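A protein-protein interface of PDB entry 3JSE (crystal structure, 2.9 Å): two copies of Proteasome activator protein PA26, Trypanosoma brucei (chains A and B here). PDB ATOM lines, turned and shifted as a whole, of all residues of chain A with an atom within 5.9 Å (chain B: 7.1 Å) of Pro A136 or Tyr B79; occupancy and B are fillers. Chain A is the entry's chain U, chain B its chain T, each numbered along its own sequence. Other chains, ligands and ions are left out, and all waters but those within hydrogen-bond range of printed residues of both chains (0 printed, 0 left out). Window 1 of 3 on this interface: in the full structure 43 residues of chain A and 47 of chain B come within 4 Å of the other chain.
The side-chain carboxylate (OE1) of Glu B126 sits at hydrogen-bond distance from the backbone NH (N) of Gly A138 (3.3 Å). The side-chain carboxylate of Glu B83 is in hydrogen-bond range of a ring nitrogen (ND1) of His A197, at 2.9 Å. The side-chain sulfur (SG) of Cys B80 lies within hydrogen-bond range of the side-chain hydroxyl (OG1) of Thr A196 (3.6 Å). The backbone carbonyl oxygen (O) of Ala A133 lies within hydrogen-bond range of the backbone NH (N) of Glu B126 (3.1 Å). N of Glu B126 lies within hydrogen-bond range of O of Thr A135, at 3.4 Å. The backbone NH (N) of Lys B127 sits at hydrogen-bond distance from the backbone carbonyl oxygen (O) of Ala A133, 3.4 Å away. The side-chain carboxylate of Glu A144 lies close to the side-chain carboxylate of Glu B126.
The side-chain hydroxyl (OG1) of Thr B84 lies within hydrogen-bond range of the backbone carbonyl oxygen (O) of Cys B80, at 3.4 Å. N of Met B139 lies close to O of Leu B122, 3.3 Å away. The side-chain hydroxyl (OH) of Tyr B140 is in hydrogen-bond range of the backbone carbonyl oxygen (O) of Ser B124. The backbone carbonyl oxygen of Glu B118 is in hydrogen-bond range of the side-chain hydroxyl of Ser B124 (3.1 Å). The side-chain hydroxyl (OG1) of Thr A135 sits at hydrogen-bond distance from the backbone carbonyl oxygen (O) of Ile A137 (3.4 Å). The backbone carbonyl oxygen (O) of His B76 sits at hydrogen-bond distance from the side-chain sulfur (SG) of Cys B80.
Ala A133 touches Gly B125. Pro A136 touches Tyr B79 (CG to OH, 3.997 Å). Pro A136 touches Ser B124. O of Pro A136 touches CG of Glu B126, 3.0 Å away. CB of Pro A136 touches OH of Tyr B140, at 3.6 Å. Ile A137 touches Glu B126. Leu A189 touches His B76. Lys A190 touches Tyr B140 (CG to OH, 3.4 Å). Met B139 touches Leu A193 (SD to CD1, 3.5 Å). Thr A196 touches Glu B83 (CG2 to CB, 3.5 Å).
Printed residues of chain B within 4 Å of Pro A136: Tyr B79 (3.997 Å), Ser B124 (3.5 Å), Glu B126 (3.0 Å) and Tyr B140 (3.6 Å). Printed residues of chain A within 4 Å of Tyr B79: Pro A136 (3.997 Å), Leu A193 (3.7 Å) and His A197 (3.2 Å). Printed residues of chain A within 4 Å of Ile B119: Pro A134 (3.97 Å). Printed residues of chain B within 4 Å of Ala A133: Gly B125, Glu B126 and Lys B127. Of the printed residues of chain B, Lys A190 touches Tyr B140. Printed residues of chain B within 4 Å of Thr A196: Cys B80 and Glu B83. The nearest printed residue of chain B that does not touch Ala A133 is Ser B124 (5.8 Å).
Printed residues of chain A that touch a printed residue of chain B: Ala A133, Pro A134, Thr A135, Pro A136, Ile A137, Gly A138, Glu A144, Leu A189, Lys A190, Leu A193, Thr A196 and His A197. Hydrophobic or aromatic side chains of chain A within 4 Å of the printed part of chain B: Ala A133, Pro A134, Pro A136, Leu A189, Leu A193 and His A197. Printed residues of chain B that touch a printed residue of chain A: His B76, Tyr B79, Cys B80, Glu B83, Ile B119, Ser B124, Gly B125, Glu B126, Lys B127, Met B139 and Tyr B140. Hydrophobic or aromatic side chains of chain B within 4 Å of the printed part of chain A: His B76, Tyr B79, Ile B119, Met B139 and Tyr B140. Among the printed residues, 25 pairs touch across the chains. Among the printed residues, no Asp or Glu carboxylate lies within 4 Å of a Lys or Arg side-chain nitrogen of the other chain.
No position is printed for both chains. Of the 25 pairs that touch across the chains among the printed residues, none has its exchanged pair printed and touching as well.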
ATOM      1  N   ALA A 133      28.855 -13.228 -22.707  1.00  0.00           N
ATOM      2  CA  ALA A 133      27.670 -14.106 -22.854  1.00  0.00           C
ATOM      3  C   ALA A 133      27.943 -15.423 -22.093  1.00  0.00           C
ATOM      4  O   ALA A 133      28.546 -16.356 -22.660  1.00  0.00           O
ATOM      5  CB  ALA A 133      27.372 -14.383 -24.338  1.00  0.00           C
ATOM      6  N   PRO A 134      27.544 -15.497 -20.795  1.00  0.00           N
ATOM      7  CA  PRO A 134      27.758 -16.768 -20.053  1.00  0.00           C
ATOM      8  C   PRO A 134      26.949 -17.943 -20.660  1.00  0.00           C
ATOM      9  O   PRO A 134      27.385 -19.116 -20.561  1.00  0.00           O
ATOM     10  CB  PRO A 134      27.283 -16.448 -18.619  1.00  0.00           C
ATOM     11  CG  PRO A 134      26.359 -15.255 -18.772  1.00  0.00           C
ATOM     12  CD  PRO A 134      26.873 -14.473 -19.964  1.00  0.00           C
ATOM     13  N   THR A 135      25.796 -17.626 -21.288  1.00  0.00           N
ATOM     14  CA  THR A 135      24.980 -18.629 -22.000  1.00  0.00           C
ATOM     15  C   THR A 135      25.714 -19.243 -23.191  1.00  0.00           C
ATOM     16  O   THR A 135      26.287 -18.501 -24.018  1.00  0.00           O
ATOM     17  CB  THR A 135      23.658 -18.062 -22.553  1.00  0.00           C
ATOM     18  OG1 THR A 135      22.909 -19.144 -23.132  1.00  0.00           O
ATOM     19  CG2 THR A 135      23.898 -16.955 -23.619  1.00  0.00           C
ATOM     20  N   PRO A 136      25.674 -20.597 -23.298  1.00  0.00           N
ATOM     21  CA  PRO A 136      26.378 -21.303 -24.403  1.00  0.00           C
ATOM     22  C   PRO A 136      26.003 -20.827 -25.848  1.00  0.00           C
ATOM     23  O   PRO A 136      26.905 -20.788 -26.719  1.00  0.00           O
ATOM     24  CB  PRO A 136      25.998 -22.779 -24.172  1.00  0.00           C
ATOM     25  CG  PRO A 136      25.593 -22.863 -22.703  1.00  0.00           C
ATOM     26  CD  PRO A 136      24.979 -21.536 -22.383  1.00  0.00           C
ATOM     27  N   ILE A 137      24.716 -20.452 -26.062  1.00  0.00           N
ATOM     28  CA  ILE A 137      24.150 -20.069 -27.396  1.00  0.00           C
ATOM     29  C   ILE A 137      22.915 -19.136 -27.315  1.00  0.00           C
ATOM     30  O   ILE A 137      22.111 -19.249 -26.408  1.00  0.00           O
ATOM     31  CB  ILE A 137      23.754 -21.332 -28.208  1.00  0.00           C
ATOM     32  CG1 ILE A 137      23.847 -21.060 -29.702  1.00  0.00           C
ATOM     33  CG2 ILE A 137      22.322 -21.845 -27.866  1.00  0.00           C
ATOM     34  CD1 ILE A 137      23.348 -22.227 -30.538  1.00  0.00           C
ATOM     35  N   GLY A 138      22.760 -18.239 -28.278  1.00  0.00           N
ATOM     36  CA  GLY A 138      21.704 -17.240 -28.221  1.00  0.00           C
ATOM     37  C   GLY A 138      20.347 -17.574 -28.827  1.00  0.00           C
ATOM     38  O   GLY A 138      20.042 -18.705 -29.128  1.00  0.00           O
ATOM     39  N   GLU A 144      24.170 -17.643 -36.189  1.00  0.00           N
ATOM     40  CA  GLU A 144      25.578 -17.823 -35.810  1.00  0.00           C
ATOM     41  C   GLU A 144      26.149 -19.068 -36.489  1.00  0.00           C
ATOM     42  O   GLU A 144      27.317 -19.065 -36.925  1.00  0.00           O
ATOM     43  CB  GLU A 144      25.759 -17.955 -34.291  1.00  0.00           C
ATOM     44  CG  GLU A 144      25.476 -16.690 -33.455  1.00  0.00           C
ATOM     45  CD  GLU A 144      25.319 -17.012 -31.939  1.00  0.00           C
ATOM     46  OE1 GLU A 144      24.318 -16.553 -31.315  1.00  0.00           O
ATOM     47  OE2 GLU A 144      26.193 -17.740 -31.377  1.00  0.00           O
ATOM     48  N   LEU A 189      25.965 -29.381 -29.363  1.00  0.00           N
ATOM     49  CA  LEU A 189      26.361 -29.405 -27.929  1.00  0.00           C
ATOM     50  C   LEU A 189      25.878 -28.130 -27.250  1.00  0.00           C
ATOM     51  O   LEU A 189      25.342 -28.143 -26.160  1.00  0.00           O
ATOM     52  CB  LEU A 189      27.897 -29.532 -27.773  1.00  0.00           C
ATOM     53  CG  LEU A 189      28.516 -29.346 -26.380  1.00  0.00           C
ATOM     54  CD1 LEU A 189      28.303 -30.571 -25.540  1.00  0.00           C
ATOM     55  CD2 LEU A 189      29.988 -29.017 -26.503  1.00  0.00           C
ATOM     56  N   LYS A 190      26.096 -27.020 -27.922  1.00  0.00           N
ATOM     57  CA  LYS A 190      25.652 -25.744 -27.420  1.00  0.00           C
ATOM     58  C   LYS A 190      24.164 -25.678 -27.155  1.00  0.00           C
ATOM     59  O   LYS A 190      23.760 -24.980 -26.265  1.00  0.00           O
ATOM     60  CB  LYS A 190      26.055 -24.635 -28.384  1.00  0.00           C
ATOM     61  CG  LYS A 190      27.558 -24.359 -28.361  1.00  0.00           C
ATOM     62  CD  LYS A 190      27.987 -23.153 -29.242  1.00  0.00           C
ATOM     63  CE  LYS A 190      29.407 -22.649 -28.848  1.00  0.00           C
ATOM     64  NZ  LYS A 190      29.930 -21.535 -29.674  1.00  0.00           N
ATOM     65  N   VAL A 191      23.349 -26.391 -27.918  1.00  0.00           N
ATOM     66  CA  VAL A 191      21.930 -26.437 -27.619  1.00  0.00           C
ATOM     67  C   VAL A 191      21.676 -27.327 -26.389  1.00  0.00           C
ATOM     68  O   VAL A 191      20.862 -26.938 -25.544  1.00  0.00           O
ATOM     69  CB  VAL A 191      21.067 -26.848 -28.829  1.00  0.00           C
ATOM     70  CG1 VAL A 191      19.561 -26.977 -28.438  1.00  0.00           C
ATOM     71  CG2 VAL A 191      21.227 -25.822 -29.919  1.00  0.00           C
ATOM     72  N   LEU A 193      23.616 -27.849 -23.813  1.00  0.00           N
ATOM     73  CA  LEU A 193      24.052 -27.027 -22.687  1.00  0.00           C
ATOM     74  C   LEU A 193      23.073 -25.870 -22.395  1.00  0.00           C
ATOM     75  O   LEU A 193      22.643 -25.666 -21.249  1.00  0.00           O
ATOM     76  CB  LEU A 193      25.448 -26.471 -22.946  1.00  0.00           C
ATOM     77  CG  LEU A 193      26.598 -27.475 -23.093  1.00  0.00           C
ATOM     78  CD1 LEU A 193      27.937 -26.723 -23.287  1.00  0.00           C
ATOM     79  CD2 LEU A 193      26.681 -28.419 -21.909  1.00  0.00           C
ATOM     80  N   ALA A 194      22.710 -25.113 -23.423  1.00  0.00           N
ATOM     81  CA  ALA A 194      21.800 -23.985 -23.229  1.00  0.00           C
ATOM     82  C   ALA A 194      20.435 -24.440 -22.733  1.00  0.00           C
ATOM     83  O   ALA A 194      19.834 -23.737 -21.929  1.00  0.00           O
ATOM     84  CB  ALA A 194      21.660 -23.167 -24.479  1.00  0.00           C
ATOM     85  N   THR A 196      19.810 -27.291 -20.847  1.00  0.00           N
ATOM     86  CA  THR A 196      20.050 -27.618 -19.418  1.00  0.00           C
ATOM     87  C   THR A 196      19.933 -26.369 -18.566  1.00  0.00           C
ATOM     88  O   THR A 196      19.147 -26.320 -17.618  1.00  0.00           O
ATOM     89  CB  THR A 196      21.463 -28.182 -19.131  1.00  0.00           C
ATOM     90  OG1 THR A 196      21.710 -29.318 -19.945  1.00  0.00           O
ATOM     91  CG2 THR A 196      21.590 -28.615 -17.704  1.00  0.00           C
ATOM     92  N   HIS A 197      20.723 -25.355 -18.924  1.00  0.00           N
ATOM     93  CA  HIS A 197      20.778 -24.097 -18.169  1.00  0.00           C
ATOM     94  C   HIS A 197      19.458 -23.285 -18.185  1.00  0.00           C
ATOM     95  O   HIS A 197      19.021 -22.761 -17.168  1.00  0.00           O
ATOM     96  CB  HIS A 197      21.951 -23.240 -18.639  1.00  0.00           C
ATOM     97  CG  HIS A 197      22.111 -21.997 -17.835  1.00  0.00           C
ATOM     98  ND1 HIS A 197      22.096 -22.000 -16.458  1.00  0.00           N
ATOM     99  CD2 HIS A 197      22.216 -20.703 -18.211  1.00  0.00           C
ATOM    100  CE1 HIS A 197      22.193 -20.762 -16.019  1.00  0.00           C
ATOM    101  NE2 HIS A 197      22.263 -19.957 -17.061  1.00  0.00           N
ATOM    102  N   TRP B  25      31.067 -37.378  -8.375  1.00  0.00           N
ATOM    103  CA  TRP B  25      32.264 -36.523  -8.480  1.00  0.00           C
ATOM    104  C   TRP B  25      33.439 -37.022  -7.597  1.00  0.00           C
ATOM    105  O   TRP B  25      34.566 -37.024  -8.034  1.00  0.00           O
ATOM    106  CB  TRP B  25      31.911 -35.054  -8.175  1.00  0.00           C
ATOM    107  CG  TRP B  25      31.132 -34.348  -9.271  1.00  0.00           C
ATOM    108  CD1 TRP B  25      30.686 -34.890 -10.410  1.00  0.00           C
ATOM    109  CD2 TRP B  25      30.677 -32.991  -9.274  1.00  0.00           C
ATOM    110  NE1 TRP B  25      30.010 -33.960 -11.150  1.00  0.00           N
ATOM    111  CE2 TRP B  25      29.976 -32.791 -10.465  1.00  0.00           C
ATOM    112  CE3 TRP B  25      30.803 -31.924  -8.382  1.00  0.00           C
ATOM    113  CZ2 TRP B  25      29.405 -31.581 -10.808  1.00  0.00           C
ATOM    114  CZ3 TRP B  25      30.228 -30.705  -8.712  1.00  0.00           C
ATOM    115  CH2 TRP B  25      29.546 -30.537  -9.923  1.00  0.00           C
ATOM    116  N   LEU B  74      33.785 -35.024 -20.891  1.00  0.00           N
ATOM    117  CA  LEU B  74      33.801 -34.833 -19.441  1.00  0.00           C
ATOM    118  C   LEU B  74      33.183 -33.484 -19.033  1.00  0.00           C
ATOM    119  O   LEU B  74      32.245 -33.435 -18.225  1.00  0.00           O
ATOM    120  CB  LEU B  74      35.212 -34.925 -18.903  1.00  0.00           C
ATOM    121  CG  LEU B  74      35.228 -34.722 -17.396  1.00  0.00           C
ATOM    122  CD1 LEU B  74      35.250 -36.045 -16.689  1.00  0.00           C
ATOM    123  CD2 LEU B  74      36.414 -33.871 -17.029  1.00  0.00           C
ATOM    124  N   CYS B  75      33.697 -32.399 -19.598  1.00  0.00           N
ATOM    125  CA  CYS B  75      33.134 -31.078 -19.349  1.00  0.00           C
ATOM    126  C   CYS B  75      31.649 -31.017 -19.618  1.00  0.00           C
ATOM    127  O   CYS B  75      30.941 -30.416 -18.838  1.00  0.00           O
ATOM    128  CB  CYS B  75      33.831 -30.000 -20.174  1.00  0.00           C
ATOM    129  SG  CYS B  75      35.578 -29.805 -19.787  1.00  0.00           S
ATOM    130  N   HIS B  76      31.169 -31.643 -20.691  1.00  0.00           N
ATOM    131  CA  HIS B  76      29.729 -31.727 -20.923  1.00  0.00           C
ATOM    132  C   HIS B  76      28.975 -32.348 -19.719  1.00  0.00           C
ATOM    133  O   HIS B  76      27.992 -31.798 -19.235  1.00  0.00           O
ATOM    134  CB  HIS B  76      29.424 -32.517 -22.181  1.00  0.00           C
ATOM    135  CG  HIS B  76      27.962 -32.724 -22.413  1.00  0.00           C
ATOM    136  ND1 HIS B  76      27.372 -33.968 -22.386  1.00  0.00           N
ATOM    137  CD2 HIS B  76      26.965 -31.841 -22.644  1.00  0.00           C
ATOM    138  CE1 HIS B  76      26.080 -33.844 -22.625  1.00  0.00           C
ATOM    139  NE2 HIS B  76      25.805 -32.561 -22.769  1.00  0.00           N
ATOM    140  N   ASN B  77      29.458 -33.464 -19.205  1.00  0.00           N
ATOM    141  CA  ASN B  77      28.785 -34.096 -18.096  1.00  0.00           C
ATOM    142  C   ASN B  77      28.854 -33.307 -16.805  1.00  0.00           C
ATOM    143  O   ASN B  77      27.835 -33.101 -16.139  1.00  0.00           O
ATOM    144  CB  ASN B  77      29.345 -35.476 -17.902  1.00  0.00           C
ATOM    145  CG  ASN B  77      29.139 -36.326 -19.115  1.00  0.00           C
ATOM    146  OD1 ASN B  77      28.217 -36.098 -19.915  1.00  0.00           O
ATOM    147  ND2 ASN B  77      30.007 -37.296 -19.286  1.00  0.00           N
ATOM    148  N   VAL B  78      30.055 -32.844 -16.459  1.00  0.00           N
ATOM    149  CA  VAL B  78      30.257 -32.036 -15.232  1.00  0.00           C
ATOM    150  C   VAL B  78      29.352 -30.783 -15.201  1.00  0.00           C
ATOM    151  O   VAL B  78      28.764 -30.458 -14.196  1.00  0.00           O
ATOM    152  CB  VAL B  78      31.732 -31.659 -15.072  1.00  0.00           C
ATOM    153  CG1 VAL B  78      31.924 -30.560 -14.051  1.00  0.00           C
ATOM    154  CG2 VAL B  78      32.524 -32.871 -14.668  1.00  0.00           C
ATOM    155  N   TYR B  79      29.208 -30.117 -16.330  1.00  0.00           N
ATOM    156  CA  TYR B  79      28.262 -29.032 -16.460  1.00  0.00           C
ATOM    157  C   TYR B  79      26.823 -29.458 -16.228  1.00  0.00           C
ATOM    158  O   TYR B  79      26.128 -28.776 -15.492  1.00  0.00           O
ATOM    159  CB  TYR B  79      28.358 -28.407 -17.840  1.00  0.00           C
ATOM    160  CG  TYR B  79      27.470 -27.197 -18.083  1.00  0.00           C
ATOM    161  CD1 TYR B  79      28.001 -25.912 -18.058  1.00  0.00           C
ATOM    162  CD2 TYR B  79      26.117 -27.342 -18.400  1.00  0.00           C
ATOM    163  CE1 TYR B  79      27.205 -24.796 -18.316  1.00  0.00           C
ATOM    164  CE2 TYR B  79      25.319 -26.246 -18.663  1.00  0.00           C
ATOM    165  CZ  TYR B  79      25.860 -24.969 -18.619  1.00  0.00           C
ATOM    166  OH  TYR B  79      25.077 -23.859 -18.867  1.00  0.00           O
ATOM    167  N   CYS B  80      26.346 -30.529 -16.863  1.00  0.00           N
ATOM    168  CA  CYS B  80      24.951 -30.934 -16.663  1.00  0.00           C
ATOM    169  C   CYS B  80      24.714 -31.330 -15.206  1.00  0.00           C
ATOM    170  O   CYS B  80      23.660 -31.054 -14.636  1.00  0.00           O
ATOM    171  CB  CYS B  80      24.543 -32.055 -17.622  1.00  0.00           C
ATOM    172  SG  CYS B  80      24.495 -31.489 -19.329  1.00  0.00           S
ATOM    173  N   GLN B  81      25.708 -31.942 -14.592  1.00  0.00           N
ATOM    174  CA  GLN B  81      25.584 -32.371 -13.211  1.00  0.00           C
ATOM    175  C   GLN B  81      25.605 -31.174 -12.243  1.00  0.00           C
ATOM    176  O   GLN B  81      24.819 -31.121 -11.301  1.00  0.00           O
ATOM    177  CB  GLN B  81      26.686 -33.382 -12.884  1.00  0.00           C
ATOM    178  CG  GLN B  81      26.614 -34.654 -13.692  1.00  0.00           C
ATOM    179  CD  GLN B  81      27.876 -35.484 -13.596  1.00  0.00           C
ATOM    180  OE1 GLN B  81      28.963 -35.035 -13.937  1.00  0.00           O
ATOM    181  NE2 GLN B  81      27.735 -36.709 -13.140  1.00  0.00           N
ATOM    182  N   ALA B  82      26.511 -30.222 -12.487  1.00  0.00           N
ATOM    183  CA  ALA B  82      26.533 -28.921 -11.796  1.00  0.00           C
ATOM    184  C   ALA B  82      25.153 -28.270 -11.811  1.00  0.00           C
ATOM    185  O   ALA B  82      24.664 -27.834 -10.786  1.00  0.00           O
ATOM    186  CB  ALA B  82      27.549 -27.998 -12.442  1.00  0.00           C
ATOM    187  N   GLU B  83      24.538 -28.231 -12.983  1.00  0.00           N
ATOM    188  CA  GLU B  83      23.202 -27.678 -13.135  1.00  0.00           C
ATOM    189  C   GLU B  83      22.121 -28.442 -12.365  1.00  0.00           C
ATOM    190  O   GLU B  83      21.112 -27.832 -11.993  1.00  0.00           O
ATOM    191  CB  GLU B  83      22.827 -27.555 -14.607  1.00  0.00           C
ATOM    192  CG  GLU B  83      23.472 -26.351 -15.298  1.00  0.00           C
ATOM    193  CD  GLU B  83      22.791 -25.043 -14.981  1.00  0.00           C
ATOM    194  OE1 GLU B  83      21.560 -24.991 -14.894  1.00  0.00           O
ATOM    195  OE2 GLU B  83      23.470 -24.031 -14.843  1.00  0.00           O
ATOM    196  N   THR B  84      22.314 -29.734 -12.100  1.00  0.00           N
ATOM    197  CA  THR B  84      21.426 -30.422 -11.155  1.00  0.00           C
ATOM    198  C   THR B  84      21.519 -29.828  -9.730  1.00  0.00           C
ATOM    199  O   THR B  84      20.494 -29.520  -9.091  1.00  0.00           O
ATOM    200  CB  THR B  84      21.681 -31.941 -11.105  1.00  0.00           C
ATOM    201  OG1 THR B  84      21.460 -32.469 -12.403  1.00  0.00           O
ATOM    202  CG2 THR B  84      20.716 -32.641 -10.122  1.00  0.00           C
ATOM    203  N   ILE B 114      29.603 -22.924  -7.744  1.00  0.00           N
ATOM    204  CA  ILE B 114      29.062 -23.653  -8.901  1.00  0.00           C
ATOM    205  C   ILE B 114      29.165 -22.775 -10.168  1.00  0.00           C
ATOM    206  O   ILE B 114      29.581 -23.236 -11.224  1.00  0.00           O
ATOM    207  CB  ILE B 114      27.630 -24.214  -8.654  1.00  0.00           C
ATOM    208  CG1 ILE B 114      27.699 -25.457  -7.759  1.00  0.00           C
ATOM    209  CG2 ILE B 114      26.971 -24.618  -9.953  1.00  0.00           C
ATOM    210  CD1 ILE B 114      26.347 -25.958  -7.343  1.00  0.00           C
ATOM    211  N   LEU B 117      32.736 -22.886 -11.302  1.00  0.00           N
ATOM    212  CA  LEU B 117      32.960 -24.168 -11.991  1.00  0.00           C
ATOM    213  C   LEU B 117      32.441 -24.147 -13.416  1.00  0.00           C
ATOM    214  O   LEU B 117      33.173 -24.480 -14.332  1.00  0.00           O
ATOM    215  CB  LEU B 117      32.287 -25.315 -11.231  1.00  0.00           C
ATOM    216  CG  LEU B 117      32.443 -26.726 -11.767  1.00  0.00           C
ATOM    217  CD1 LEU B 117      33.845 -27.177 -11.445  1.00  0.00           C
ATOM    218  CD2 LEU B 117      31.400 -27.640 -11.133  1.00  0.00           C
ATOM    219  N   GLU B 118      31.183 -23.760 -13.595  1.00  0.00           N
ATOM    220  CA  GLU B 118      30.546 -23.828 -14.910  1.00  0.00           C
ATOM    221  C   GLU B 118      31.153 -22.816 -15.878  1.00  0.00           C
ATOM    222  O   GLU B 118      31.586 -23.163 -16.971  1.00  0.00           O
ATOM    223  CB  GLU B 118      29.031 -23.600 -14.792  1.00  0.00           C
ATOM    224  CG  GLU B 118      28.267 -24.661 -13.953  1.00  0.00           C
ATOM    225  CD  GLU B 118      26.769 -24.562 -14.116  1.00  0.00           C
ATOM    226  OE1 GLU B 118      26.346 -24.370 -15.251  1.00  0.00           O
ATOM    227  OE2 GLU B 118      26.013 -24.661 -13.145  1.00  0.00           O
ATOM    228  N   ILE B 119      31.170 -21.557 -15.469  1.00  0.00           N
ATOM    229  CA  ILE B 119      31.551 -20.458 -16.358  1.00  0.00           C
ATOM    230  C   ILE B 119      33.066 -20.385 -16.450  1.00  0.00           C
ATOM    231  O   ILE B 119      33.639 -20.733 -17.461  1.00  0.00           O
ATOM    232  CB  ILE B 119      30.904 -19.079 -15.907  1.00  0.00           C
ATOM    233  CG1 ILE B 119      29.374 -19.078 -16.188  1.00  0.00           C
ATOM    234  CG2 ILE B 119      31.603 -17.890 -16.582  1.00  0.00           C
ATOM    235  CD1 ILE B 119      28.561 -18.179 -15.284  1.00  0.00           C
ATOM    236  N   LEU B 122      34.828 -24.592 -16.683  1.00  0.00           N
ATOM    237  CA  LEU B 122      34.435 -25.311 -17.893  1.00  0.00           C
ATOM    238  C   LEU B 122      34.359 -24.391 -19.112  1.00  0.00           C
ATOM    239  O   LEU B 122      34.006 -24.852 -20.195  1.00  0.00           O
ATOM    240  CB  LEU B 122      33.097 -26.048 -17.712  1.00  0.00           C
ATOM    241  CG  LEU B 122      33.009 -27.084 -16.589  1.00  0.00           C
ATOM    242  CD1 LEU B 122      31.589 -27.566 -16.462  1.00  0.00           C
ATOM    243  CD2 LEU B 122      33.962 -28.262 -16.790  1.00  0.00           C
ATOM    244  N   SER B 124      32.359 -22.400 -20.540  1.00  0.00           N
ATOM    245  CA  SER B 124      31.208 -22.896 -21.308  1.00  0.00           C
ATOM    246  C   SER B 124      30.370 -21.840 -22.076  1.00  0.00           C
ATOM    247  O   SER B 124      29.358 -22.193 -22.721  1.00  0.00           O
ATOM    248  CB  SER B 124      30.280 -23.687 -20.372  1.00  0.00           C
ATOM    249  OG  SER B 124      29.669 -22.833 -19.400  1.00  0.00           O
ATOM    250  N   GLY B 125      30.774 -20.566 -22.015  1.00  0.00           N
ATOM    251  CA  GLY B 125      29.994 -19.468 -22.632  1.00  0.00           C
ATOM    252  C   GLY B 125      30.429 -19.134 -24.048  1.00  0.00           C
ATOM    253  O   GLY B 125      31.516 -19.532 -24.462  1.00  0.00           O
ATOM    254  N   GLU B 126      29.566 -18.433 -24.795  1.00  0.00           N
ATOM    255  CA  GLU B 126      29.924 -17.872 -26.126  1.00  0.00           C
ATOM    256  C   GLU B 126      31.110 -16.911 -25.990  1.00  0.00           C
ATOM    257  O   GLU B 126      32.070 -16.947 -26.778  1.00  0.00           O
ATOM    258  CB  GLU B 126      28.751 -17.086 -26.756  1.00  0.00           C
ATOM    259  CG  GLU B 126      27.547 -17.940 -27.194  1.00  0.00           C
ATOM    260  CD  GLU B 126      26.218 -17.154 -27.256  1.00  0.00           C
ATOM    261  OE1 GLU B 126      25.770 -16.834 -28.394  1.00  0.00           O
ATOM    262  OE2 GLU B 126      25.627 -16.862 -26.170  1.00  0.00           O
ATOM    263  N   LYS B 127      31.015 -16.039 -24.988  1.00  0.00           N
ATOM    264  CA  LYS B 127      32.040 -15.031 -24.722  1.00  0.00           C
ATOM    265  C   LYS B 127      32.525 -15.064 -23.255  1.00  0.00           C
ATOM    266  O   LYS B 127      31.757 -15.407 -22.326  1.00  0.00           O
ATOM    267  CB  LYS B 127      31.534 -13.616 -25.126  1.00  0.00           C
ATOM    268  CG  LYS B 127      31.469 -13.390 -26.669  1.00  0.00           C
ATOM    269  CD  LYS B 127      31.436 -11.903 -27.097  1.00  0.00           C
ATOM    270  CE  LYS B 127      31.881 -11.762 -28.554  1.00  0.00           C
ATOM    271  NZ  LYS B 127      31.327 -10.533 -29.177  1.00  0.00           N
ATOM    272  N   MET B 139      35.295 -25.709 -23.139  1.00  0.00           N
ATOM    273  CA  MET B 139      34.472 -26.804 -23.665  1.00  0.00           C
ATOM    274  C   MET B 139      34.655 -26.927 -25.173  1.00  0.00           C
ATOM    275  O   MET B 139      34.576 -28.023 -25.737  1.00  0.00           O
ATOM    276  CB  MET B 139      32.974 -26.559 -23.396  1.00  0.00           C
ATOM    277  CG  MET B 139      32.489 -27.053 -22.055  1.00  0.00           C
ATOM    278  SD  MET B 139      31.047 -28.036 -22.193  1.00  0.00           S
ATOM    279  CE  MET B 139      31.489 -29.111 -23.550  1.00  0.00           C
ATOM    280  N   TYR B 140      34.880 -25.794 -25.832  1.00  0.00           N
ATOM    281  CA  TYR B 140      34.987 -25.774 -27.278  1.00  0.00           C
ATOM    282  C   TYR B 140      36.464 -25.752 -27.682  1.00  0.00           C
ATOM    283  O   TYR B 140      36.853 -25.027 -28.601  1.00  0.00           O
ATOM    284  CB  TYR B 140      34.211 -24.580 -27.840  1.00  0.00           C
ATOM    285  CG  TYR B 140      32.834 -24.432 -27.210  1.00  0.00           C
ATOM    286  CD1 TYR B 140      32.510 -23.298 -26.475  1.00  0.00           C
ATOM    287  CD2 TYR B 140      31.871 -25.454 -27.316  1.00  0.00           C
ATOM    288  CE1 TYR B 140      31.270 -23.171 -25.877  1.00  0.00           C
ATOM    289  CE2 TYR B 140      30.630 -25.336 -26.721  1.00  0.00           C
ATOM    290  CZ  TYR B 140      30.339 -24.188 -26.000  1.00  0.00           C
ATOM    291  OH  TYR B 140      29.115 -24.040 -25.392  1.00  0.00           O
